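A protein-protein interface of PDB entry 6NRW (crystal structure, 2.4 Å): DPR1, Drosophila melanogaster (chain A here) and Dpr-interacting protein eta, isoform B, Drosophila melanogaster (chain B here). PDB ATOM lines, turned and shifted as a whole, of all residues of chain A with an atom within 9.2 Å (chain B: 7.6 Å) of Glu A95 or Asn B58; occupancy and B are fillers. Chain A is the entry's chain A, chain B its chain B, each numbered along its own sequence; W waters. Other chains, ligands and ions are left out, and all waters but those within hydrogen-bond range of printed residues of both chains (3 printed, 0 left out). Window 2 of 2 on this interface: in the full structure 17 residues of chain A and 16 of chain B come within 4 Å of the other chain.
The side-chain amide nitrogen (ND2) of Asn A93 is in hydrogen-bond range of the backbone carbonyl oxygen (O) of Ile B55 (2.9 Å). The backbone carbonyl oxygen (O) of Asn A93 lies within hydrogen-bond range of the backbone NH (N) of Lys B57, at 3.2 Å. ND2 of Asn B58 sits at hydrogen-bond distance from OE2 of Glu A95, 3.4 Å away.
N of Arg B41 lies within hydrogen-bond range of O of Thr B46 (2.9 Å). N of Ile B55 is in hydrogen-bond range of O of Leu B48. The backbone NH (N) of Asn B58 sits at hydrogen-bond distance from the side-chain hydroxyl (OG1) of Thr B56, at 3.0 Å. The side-chain amide oxygen of Asn B58 is in hydrogen-bond range of the backbone NH of Arg B60, at 2.9 Å.
Among the printed residues, pairs that only touch across the chains: Lys A97 with Thr B46 (3.5 Å) and Lys A36 with Lys B57 (3.8 Å).
Printed residues of chain B within 4 Å of Lys A36: Lys B57 (3.8 Å). Of the printed residues of chain B, Asn A93 touches Ile B55 (2.9 Å) and Lys B57 (3.2 Å). Glu A95 touches one residue of chain B. Of chain A, only Glu A95 (3.4 Å) comes within 4 Å of Asn B58. Ile B61 touches none of the printed residues of chain A. Asp B77 touches none of the printed residues of chain A. The nearest residue of chain B that does not touch Glu A95 is Thr B56 (4.3 Å).
Printed residues of chain A that touch a printed residue of chain B: Lys A36, Asn A93, Glu A95 and Lys A97. Of the 20 printed residues of chain B, 4 touch a printed residue of chain A. Hydrophobic or aromatic side chains of chain B within 4 Å of the printed part of chain A: Ile B55. Along chain B the printed residues that touch a printed residue of chain A span positions 46 to 58. Among the printed residues, no Asp or Glu carboxylate lies within 4 Å of a Lys or Arg side-chain nitrogen of the other chain.
Water W1 lies within hydrogen-bond range of O of Thr A94 (2.6 Å) and OG1 of Thr B56 (2.8 Å). Water W3 bridges the side-chain hydroxyl of Thr B46 and the backbone NH of Lys A97. Water W2 lies within hydrogen-bond range of the side-chain carboxylate (OE2) of Glu A95 and the guanidinium group (NH2) of Arg B60.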
ATOM      1  N   PRO A   3     -15.910 -37.420   1.781  1.00  0.00           N
ATOM      2  CA  PRO A   3     -14.553 -37.269   1.227  1.00  0.00           C
ATOM      3  C   PRO A   3     -13.462 -37.197   2.282  1.00  0.00           C
ATOM      4  O   PRO A   3     -12.282 -37.335   1.930  1.00  0.00           O
ATOM      5  CB  PRO A   3     -14.642 -35.958   0.438  1.00  0.00           C
ATOM      6  CG  PRO A   3     -15.747 -35.197   1.104  1.00  0.00           C
ATOM      7  CD  PRO A   3     -16.742 -36.224   1.564  1.00  0.00           C
ATOM      8  N   LEU A   5     -12.265 -34.685   3.842  1.00  0.00           N
ATOM      9  CA  LEU A   5     -11.425 -33.521   3.647  1.00  0.00           C
ATOM     10  C   LEU A   5     -11.160 -32.860   4.995  1.00  0.00           C
ATOM     11  O   LEU A   5     -11.774 -33.213   6.002  1.00  0.00           O
ATOM     12  CB  LEU A   5     -12.099 -32.557   2.672  1.00  0.00           C
ATOM     13  CG  LEU A   5     -12.217 -33.132   1.260  1.00  0.00           C
ATOM     14  CD1 LEU A   5     -12.965 -32.184   0.335  1.00  0.00           C
ATOM     15  CD2 LEU A   5     -10.834 -33.431   0.715  1.00  0.00           C
ATOM     16  N   PRO A   6     -10.232 -31.910   5.058  1.00  0.00           N
ATOM     17  CA  PRO A   6     -10.076 -31.129   6.288  1.00  0.00           C
ATOM     18  C   PRO A   6     -11.289 -30.241   6.516  1.00  0.00           C
ATOM     19  O   PRO A   6     -12.158 -30.081   5.655  1.00  0.00           O
ATOM     20  CB  PRO A   6      -8.814 -30.299   6.034  1.00  0.00           C
ATOM     21  CG  PRO A   6      -8.061 -31.072   4.997  1.00  0.00           C
ATOM     22  CD  PRO A   6      -9.120 -31.677   4.121  1.00  0.00           C
ATOM     23  N   LYS A  36      -3.013 -32.497   3.058  1.00  0.00           N
ATOM     24  CA  LYS A  36      -3.244 -31.157   2.548  1.00  0.00           C
ATOM     25  C   LYS A  36      -2.284 -30.169   3.212  1.00  0.00           C
ATOM     26  O   LYS A  36      -1.505 -30.519   4.099  1.00  0.00           O
ATOM     27  CB  LYS A  36      -4.693 -30.745   2.803  1.00  0.00           C
ATOM     28  CG  LYS A  36      -5.750 -31.680   2.220  1.00  0.00           C
ATOM     29  CD  LYS A  36      -5.521 -32.098   0.779  1.00  0.00           C
ATOM     30  CE  LYS A  36      -6.494 -33.231   0.427  1.00  0.00           C
ATOM     31  NZ  LYS A  36      -6.568 -33.557  -1.025  1.00  0.00           N
ATOM     32  N   ILE A  92      -6.879 -23.822   2.248  1.00  0.00           N
ATOM     33  CA  ILE A  92      -6.430 -25.209   2.200  1.00  0.00           C
ATOM     34  C   ILE A  92      -6.320 -25.621   0.739  1.00  0.00           C
ATOM     35  O   ILE A  92      -7.195 -25.296  -0.072  1.00  0.00           O
ATOM     36  CB  ILE A  92      -7.410 -26.130   2.959  1.00  0.00           C
ATOM     37  CG1 ILE A  92      -7.685 -25.588   4.362  1.00  0.00           C
ATOM     38  CG2 ILE A  92      -6.882 -27.559   3.022  1.00  0.00           C
ATOM     39  CD1 ILE A  92      -8.692 -26.401   5.147  1.00  0.00           C
ATOM     40  N   ASN A  93      -5.255 -26.354   0.404  1.00  0.00           N
ATOM     41  CA  ASN A  93      -4.932 -26.625  -0.994  1.00  0.00           C
ATOM     42  C   ASN A  93      -5.740 -27.772  -1.602  1.00  0.00           C
ATOM     43  O   ASN A  93      -5.252 -28.474  -2.495  1.00  0.00           O
ATOM     44  CB  ASN A  93      -3.427 -26.874  -1.147  1.00  0.00           C
ATOM     45  CG  ASN A  93      -2.951 -28.098  -0.400  1.00  0.00           C
ATOM     46  OD1 ASN A  93      -3.644 -28.616   0.476  1.00  0.00           O
ATOM     47  ND2 ASN A  93      -1.750 -28.562  -0.737  1.00  0.00           N
ATOM     48  N   THR A  94      -6.968 -27.978  -1.124  1.00  0.00           N
ATOM     49  CA  THR A  94      -7.878 -28.920  -1.764  1.00  0.00           C
ATOM     50  C   THR A  94      -8.293 -28.416  -3.147  1.00  0.00           C
ATOM     51  O   THR A  94      -8.052 -27.269  -3.526  1.00  0.00           O
ATOM     52  CB  THR A  94      -9.128 -29.145  -0.915  1.00  0.00           C
ATOM     53  OG1 THR A  94      -9.781 -27.888  -0.692  1.00  0.00           O
ATOM     54  CG2 THR A  94      -8.774 -29.790   0.413  1.00  0.00           C
ATOM     55  N   GLU A  95      -8.925 -29.305  -3.904  1.00  0.00           N
ATOM     56  CA  GLU A  95      -9.395 -29.006  -5.256  1.00  0.00           C
ATOM     57  C   GLU A  95     -10.911 -29.164  -5.316  1.00  0.00           C
ATOM     58  O   GLU A  95     -11.417 -30.300  -5.359  1.00  0.00           O
ATOM     59  CB  GLU A  95      -8.702 -29.933  -6.257  1.00  0.00           C
ATOM     60  CG  GLU A  95      -9.337 -30.065  -7.636  1.00  0.00           C
ATOM     61  CD  GLU A  95      -9.264 -28.797  -8.461  1.00  0.00           C
ATOM     62  OE1 GLU A  95      -8.702 -27.788  -7.980  1.00  0.00           O
ATOM     63  OE2 GLU A  95      -9.760 -28.819  -9.607  1.00  0.00           O
ATOM     64  N   PRO A  96     -11.689 -28.067  -5.312  1.00  0.00           N
ATOM     65  CA  PRO A  96     -11.277 -26.660  -5.234  1.00  0.00           C
ATOM     66  C   PRO A  96     -10.856 -26.283  -3.820  1.00  0.00           C
ATOM     67  O   PRO A  96     -11.079 -27.064  -2.892  1.00  0.00           O
ATOM     68  CB  PRO A  96     -12.550 -25.890  -5.636  1.00  0.00           C
ATOM     69  CG  PRO A  96     -13.542 -26.937  -6.090  1.00  0.00           C
ATOM     70  CD  PRO A  96     -13.152 -28.185  -5.368  1.00  0.00           C
ATOM     71  N   LYS A  97     -10.290 -25.089  -3.658  1.00  0.00           N
ATOM     72  CA  LYS A  97      -9.759 -24.690  -2.363  1.00  0.00           C
ATOM     73  C   LYS A  97     -10.861 -24.617  -1.310  1.00  0.00           C
ATOM     74  O   LYS A  97     -12.052 -24.487  -1.605  1.00  0.00           O
ATOM     75  CB  LYS A  97      -9.067 -23.325  -2.451  1.00  0.00           C
ATOM     76  CG  LYS A  97     -10.035 -22.148  -2.557  1.00  0.00           C
ATOM     77  CD  LYS A  97      -9.346 -20.795  -2.411  1.00  0.00           C
ATOM     78  CE  LYS A  97     -10.375 -19.666  -2.440  1.00  0.00           C
ATOM     79  NZ  LYS A  97      -9.760 -18.299  -2.498  1.00  0.00           N
ATOM     80  N   MET A  98     -10.438 -24.724  -0.060  1.00  0.00           N
ATOM     81  CA  MET A  98     -11.229 -24.319   1.088  1.00  0.00           C
ATOM     82  C   MET A  98     -10.617 -23.040   1.634  1.00  0.00           C
ATOM     83  O   MET A  98      -9.391 -22.902   1.668  1.00  0.00           O
ATOM     84  CB  MET A  98     -11.259 -25.403   2.166  1.00  0.00           C
ATOM     85  CG  MET A  98     -12.046 -26.632   1.768  1.00  0.00           C
ATOM     86  SD  MET A  98     -11.971 -27.928   3.010  1.00  0.00           S
ATOM     87  CE  MET A  98     -13.123 -29.109   2.318  1.00  0.00           C
ATOM     88  N   ARG B  41      -4.149 -18.813  -9.509  1.00  0.00           N
ATOM     89  CA  ARG B  41      -5.376 -18.549 -10.247  1.00  0.00           C
ATOM     90  C   ARG B  41      -6.006 -17.276  -9.694  1.00  0.00           C
ATOM     91  O   ARG B  41      -6.315 -17.202  -8.500  1.00  0.00           O
ATOM     92  CB  ARG B  41      -6.344 -19.724 -10.143  1.00  0.00           C
ATOM     93  CG  ARG B  41      -7.667 -19.482 -10.858  1.00  0.00           C
ATOM     94  CD  ARG B  41      -7.547 -19.857 -12.321  1.00  0.00           C
ATOM     95  NE  ARG B  41      -8.764 -19.599 -13.084  1.00  0.00           N
ATOM     96  CZ  ARG B  41      -9.698 -20.511 -13.325  1.00  0.00           C
ATOM     97  NH1 ARG B  41      -9.560 -21.744 -12.857  1.00  0.00           N
ATOM     98  NH2 ARG B  41     -10.770 -20.193 -14.034  1.00  0.00           N
ATOM     99  N   THR B  46      -6.439 -18.803  -5.866  1.00  0.00           N
ATOM    100  CA  THR B  46      -5.933 -20.095  -5.428  1.00  0.00           C
ATOM    101  C   THR B  46      -4.446 -20.191  -5.738  1.00  0.00           C
ATOM    102  O   THR B  46      -4.022 -19.902  -6.864  1.00  0.00           O
ATOM    103  CB  THR B  46      -6.700 -21.234  -6.107  1.00  0.00           C
ATOM    104  OG1 THR B  46      -8.077 -21.202  -5.696  1.00  0.00           O
ATOM    105  CG2 THR B  46      -6.094 -22.579  -5.733  1.00  0.00           C
ATOM    106  N   LEU B  48      -1.350 -22.005  -6.858  1.00  0.00           N
ATOM    107  CA  LEU B  48      -1.117 -23.178  -7.697  1.00  0.00           C
ATOM    108  C   LEU B  48       0.281 -23.767  -7.500  1.00  0.00           C
ATOM    109  O   LEU B  48       0.411 -24.950  -7.164  1.00  0.00           O
ATOM    110  CB  LEU B  48      -1.361 -22.824  -9.170  1.00  0.00           C
ATOM    111  CG  LEU B  48      -2.748 -22.270  -9.512  1.00  0.00           C
ATOM    112  CD1 LEU B  48      -2.844 -21.906 -10.989  1.00  0.00           C
ATOM    113  CD2 LEU B  48      -3.842 -23.251  -9.129  1.00  0.00           C
ATOM    114  N   VAL B  54       4.360 -27.942  -6.859  1.00  0.00           N
ATOM    115  CA  VAL B  54       2.944 -27.699  -7.110  1.00  0.00           C
ATOM    116  C   VAL B  54       2.223 -27.724  -5.770  1.00  0.00           C
ATOM    117  O   VAL B  54       2.273 -28.725  -5.051  1.00  0.00           O
ATOM    118  CB  VAL B  54       2.362 -28.746  -8.073  1.00  0.00           C
ATOM    119  CG1 VAL B  54       0.895 -28.449  -8.360  1.00  0.00           C
ATOM    120  CG2 VAL B  54       3.164 -28.795  -9.365  1.00  0.00           C
ATOM    121  N   ILE B  55       1.558 -26.623  -5.428  1.00  0.00           N
ATOM    122  CA  ILE B  55       0.836 -26.543  -4.160  1.00  0.00           C
ATOM    123  C   ILE B  55      -0.561 -27.133  -4.285  1.00  0.00           C
ATOM    124  O   ILE B  55      -1.001 -27.899  -3.423  1.00  0.00           O
ATOM    125  CB  ILE B  55       0.785 -25.087  -3.643  1.00  0.00           C
ATOM    126  CG1 ILE B  55       2.042 -24.741  -2.839  1.00  0.00           C
ATOM    127  CG2 ILE B  55      -0.432 -24.884  -2.748  1.00  0.00           C
ATOM    128  CD1 ILE B  55       3.292 -24.684  -3.647  1.00  0.00           C
ATOM    129  N   THR B  56      -1.275 -26.795  -5.354  1.00  0.00           N
ATOM    130  CA  THR B  56      -2.628 -27.304  -5.508  1.00  0.00           C
ATOM    131  C   THR B  56      -2.612 -28.821  -5.642  1.00  0.00           C
ATOM    132  O   THR B  56      -1.698 -29.410  -6.226  1.00  0.00           O
ATOM    133  CB  THR B  56      -3.311 -26.683  -6.728  1.00  0.00           C
ATOM    134  OG1 THR B  56      -4.596 -27.291  -6.917  1.00  0.00           O
ATOM    135  CG2 THR B  56      -2.468 -26.888  -7.982  1.00  0.00           C
ATOM    136  N   LYS B  57      -3.641 -29.450  -5.083  1.00  0.00           N
ATOM    137  CA  LYS B  57      -3.845 -30.879  -5.245  1.00  0.00           C
ATOM    138  C   LYS B  57      -4.488 -31.221  -6.579  1.00  0.00           C
ATOM    139  O   LYS B  57      -4.767 -32.397  -6.834  1.00  0.00           O
ATOM    140  CB  LYS B  57      -4.685 -31.428  -4.093  1.00  0.00           C
ATOM    141  CG  LYS B  57      -3.949 -31.434  -2.769  1.00  0.00           C
ATOM    142  CD  LYS B  57      -2.689 -32.276  -2.871  1.00  0.00           C
ATOM    143  CE  LYS B  57      -2.022 -32.455  -1.520  1.00  0.00           C
ATOM    144  NZ  LYS B  57      -0.874 -33.406  -1.593  1.00  0.00           N
ATOM    145  N   ASN B  58      -4.751 -30.221  -7.417  1.00  0.00           N
ATOM    146  CA  ASN B  58      -5.146 -30.461  -8.798  1.00  0.00           C
ATOM    147  C   ASN B  58      -4.004 -31.162  -9.524  1.00  0.00           C
ATOM    148  O   ASN B  58      -2.982 -30.543  -9.842  1.00  0.00           O
ATOM    149  CB  ASN B  58      -5.506 -29.140  -9.480  1.00  0.00           C
ATOM    150  CG  ASN B  58      -6.134 -29.333 -10.849  1.00  0.00           C
ATOM    151  OD1 ASN B  58      -5.937 -30.360 -11.504  1.00  0.00           O
ATOM    152  ND2 ASN B  58      -6.895 -28.335 -11.292  1.00  0.00           N
ATOM    153  N   GLN B  59      -4.171 -32.452  -9.802  1.00  0.00           N
ATOM    154  CA  GLN B  59      -3.098 -33.221 -10.417  1.00  0.00           C
ATOM    155  C   GLN B  59      -2.854 -32.852 -11.874  1.00  0.00           C
ATOM    156  O   GLN B  59      -1.874 -33.327 -12.454  1.00  0.00           O
ATOM    157  CB  GLN B  59      -3.397 -34.715 -10.311  1.00  0.00           C
ATOM    158  CG  GLN B  59      -3.236 -35.281  -8.913  1.00  0.00           C
ATOM    159  CD  GLN B  59      -3.267 -36.799  -8.901  1.00  0.00           C
ATOM    160  OE1 GLN B  59      -3.766 -37.427  -9.836  1.00  0.00           O
ATOM    161  NE2 GLN B  59      -2.722 -37.397  -7.846  1.00  0.00           N
ATOM    162  N   ARG B  60      -3.717 -32.038 -12.477  1.00  0.00           N
ATOM    163  CA  ARG B  60      -3.504 -31.580 -13.845  1.00  0.00           C
ATOM    164  C   ARG B  60      -2.490 -30.446 -13.947  1.00  0.00           C
ATOM    165  O   ARG B  60      -2.205 -29.993 -15.061  1.00  0.00           O
ATOM    166  CB  ARG B  60      -4.831 -31.134 -14.469  1.00  0.00           C
ATOM    167  CG  ARG B  60      -5.879 -32.230 -14.555  1.00  0.00           C
ATOM    168  CD  ARG B  60      -7.160 -31.725 -15.203  1.00  0.00           C
ATOM    169  NE  ARG B  60      -7.738 -30.598 -14.475  1.00  0.00           N
ATOM    170  CZ  ARG B  60      -7.864 -29.373 -14.976  1.00  0.00           C
ATOM    171  NH1 ARG B  60      -7.464 -29.119 -16.215  1.00  0.00           N
ATOM    172  NH2 ARG B  60      -8.396 -28.406 -14.244  1.00  0.00           N
ATOM    173  N   ILE B  61      -1.939 -29.980 -12.828  1.00  0.00           N
ATOM    174  CA  ILE B  61      -1.066 -28.812 -12.805  1.00  0.00           C
ATOM    175  C   ILE B  61       0.363 -29.239 -12.488  1.00  0.00           C
ATOM    176  O   ILE B  61       0.610 -29.926 -11.488  1.00  0.00           O
ATOM    177  CB  ILE B  61      -1.569 -27.763 -11.799  1.00  0.00           C
ATOM    178  CG1 ILE B  61      -2.831 -27.086 -12.341  1.00  0.00           C
ATOM    179  CG2 ILE B  61      -0.479 -26.741 -11.490  1.00  0.00           C
ATOM    180  CD1 ILE B  61      -3.361 -25.993 -11.461  1.00  0.00           C
ATOM    181  N   GLY B  62       1.301 -28.824 -13.344  1.00  0.00           N
ATOM    182  CA  GLY B  62       2.710 -29.036 -13.096  1.00  0.00           C
ATOM    183  C   GLY B  62       3.494 -27.767 -13.368  1.00  0.00           C
ATOM    184  O   GLY B  62       3.009 -26.835 -14.013  1.00  0.00           O
ATOM    185  N   ARG B  74       2.184 -25.837 -16.560  1.00  0.00           N
ATOM    186  CA  ARG B  74       1.431 -26.660 -17.488  1.00  0.00           C
ATOM    187  C   ARG B  74       0.109 -27.072 -16.854  1.00  0.00           C
ATOM    188  O   ARG B  74       0.049 -27.356 -15.652  1.00  0.00           O
ATOM    189  CB  ARG B  74       2.238 -27.892 -17.886  1.00  0.00           C
ATOM    190  CG  ARG B  74       1.465 -28.902 -18.680  1.00  0.00           C
ATOM    191  CD  ARG B  74       2.284 -30.154 -18.852  1.00  0.00           C
ATOM    192  NE  ARG B  74       1.550 -31.184 -19.570  1.00  0.00           N
ATOM    193  CZ  ARG B  74       1.929 -32.454 -19.625  1.00  0.00           C
ATOM    194  NH1 ARG B  74       3.030 -32.841 -18.994  1.00  0.00           N
ATOM    195  NH2 ARG B  74       1.205 -33.334 -20.304  1.00  0.00           N
ATOM    196  N   ILE B  75      -0.951 -27.080 -17.659  1.00  0.00           N
ATOM    197  CA  ILE B  75      -2.278 -27.510 -17.233  1.00  0.00           C
ATOM    198  C   ILE B  75      -2.716 -28.637 -18.163  1.00  0.00           C
ATOM    199  O   ILE B  75      -3.040 -28.393 -19.332  1.00  0.00           O
ATOM    200  CB  ILE B  75      -3.289 -26.356 -17.250  1.00  0.00           C
ATOM    201  CG1 ILE B  75      -2.807 -25.196 -16.374  1.00  0.00           C
ATOM    202  CG2 ILE B  75      -4.652 -26.837 -16.768  1.00  0.00           C
ATOM    203  CD1 ILE B  75      -3.694 -23.967 -16.441  1.00  0.00           C
ATOM    204  N   LYS B  76      -2.700 -29.873 -17.656  1.00  0.00           N
ATOM    205  CA  LYS B  76      -3.147 -31.028 -18.432  1.00  0.00           C
ATOM    206  C   LYS B  76      -4.659 -31.006 -18.634  1.00  0.00           C
ATOM    207  O   LYS B  76      -5.403 -30.433 -17.834  1.00  0.00           O
ATOM    208  CB  LYS B  76      -2.758 -32.340 -17.742  1.00  0.00           C
ATOM    209  CG  LYS B  76      -1.276 -32.673 -17.746  1.00  0.00           C
ATOM    210  CD  LYS B  76      -0.977 -33.873 -16.841  1.00  0.00           C
ATOM    211  CE  LYS B  76       0.362 -34.520 -17.199  1.00  0.00           C
ATOM    212  NZ  LYS B  76       0.747 -35.633 -16.279  1.00  0.00           N
ATOM    213  N   ASP B  77      -5.102 -31.629 -19.735  1.00  0.00           N
ATOM    214  CA  ASP B  77      -6.508 -31.949 -19.988  1.00  0.00           C
ATOM    215  C   ASP B  77      -7.421 -30.782 -19.647  1.00  0.00           C
ATOM    216  O   ASP B  77      -8.167 -30.838 -18.665  1.00  0.00           O
ATOM    217  CB  ASP B  77      -6.910 -33.197 -19.193  1.00  0.00           C
ATOM    218  CG  ASP B  77      -8.189 -33.844 -19.711  1.00  0.00           C
ATOM    219  OD1 ASP B  77      -8.448 -33.764 -20.932  1.00  0.00           O
ATOM    220  OD2 ASP B  77      -8.935 -34.437 -18.896  1.00  0.00           O
ATOM    221  N   LYS B  79     -10.131 -28.105 -18.958  1.00  0.00           N
ATOM    222  CA  LYS B  79     -11.560 -27.983 -18.736  1.00  0.00           C
ATOM    223  C   LYS B  79     -11.973 -26.541 -19.010  1.00  0.00           C
ATOM    224  O   LYS B  79     -11.167 -25.617 -18.872  1.00  0.00           O
ATOM    225  CB  LYS B  79     -11.899 -28.367 -17.297  1.00  0.00           C
ATOM    226  CG  LYS B  79     -11.275 -29.687 -16.841  1.00  0.00           C
ATOM    227  CD  LYS B  79     -11.707 -30.859 -17.707  1.00  0.00           C
ATOM    228  CE  LYS B  79     -11.224 -32.194 -17.138  1.00  0.00           C
ATOM    229  NZ  LYS B  79      -9.752 -32.380 -17.246  1.00  0.00           N
ATOM    230  N   SER B  81     -13.693 -24.718 -17.262  1.00  0.00           N
ATOM    231  CA  SER B  81     -13.524 -24.011 -15.997  1.00  0.00           C
ATOM    232  C   SER B  81     -12.095 -23.540 -15.750  1.00  0.00           C
ATOM    233  O   SER B  81     -11.863 -22.821 -14.772  1.00  0.00           O
ATOM    234  CB  SER B  81     -13.994 -24.906 -14.848  1.00  0.00           C
ATOM    235  OG  SER B  81     -13.409 -26.195 -14.932  1.00  0.00           O
ATOM    236  N   ASP B  82     -11.128 -23.944 -16.579  1.00  0.00           N
ATOM    237  CA  ASP B  82      -9.773 -23.418 -16.448  1.00  0.00           C
ATOM    238  C   ASP B  82      -9.616 -22.027 -17.052  1.00  0.00           C
ATOM    239  O   ASP B  82      -8.627 -21.348 -16.754  1.00  0.00           O
ATOM    240  CB  ASP B  82      -8.762 -24.359 -17.110  1.00  0.00           C
ATOM    241  CG  ASP B  82      -8.612 -25.676 -16.374  1.00  0.00           C
ATOM    242  OD1 ASP B  82      -8.625 -25.664 -15.127  1.00  0.00           O
ATOM    243  OD2 ASP B  82      -8.476 -26.722 -17.046  1.00  0.00           O
ATOM    244  N   TYR B  86      -4.449 -15.770 -14.710  1.00  0.00           N
ATOM    245  CA  TYR B  86      -3.435 -16.418 -13.895  1.00  0.00           C
ATOM    246  C   TYR B  86      -2.345 -15.411 -13.571  1.00  0.00           C
ATOM    247  O   TYR B  86      -1.969 -14.597 -14.419  1.00  0.00           O
ATOM    248  CB  TYR B  86      -2.853 -17.642 -14.611  1.00  0.00           C
ATOM    249  CG  TYR B  86      -3.856 -18.769 -14.754  1.00  0.00           C
ATOM    250  CD1 TYR B  86      -4.837 -18.740 -15.742  1.00  0.00           C
ATOM    251  CD2 TYR B  86      -3.831 -19.855 -13.886  1.00  0.00           C
ATOM    252  CE1 TYR B  86      -5.759 -19.765 -15.865  1.00  0.00           C
ATOM    253  CE2 TYR B  86      -4.745 -20.881 -14.001  1.00  0.00           C
ATOM    254  CZ  TYR B  86      -5.707 -20.831 -14.990  1.00  0.00           C
ATOM    255  OH  TYR B  86      -6.621 -21.855 -15.104  1.00  0.00           O
HETATM  256  O   HOH W   1      -6.254 -26.045  -5.002  1.00  0.00           O
HETATM  257  O   HOH W   2     -10.507 -29.812 -12.104  1.00  0.00           O
HETATM  258  O   HOH W   3      -9.487 -23.468  -6.241  1.00  0.00           O
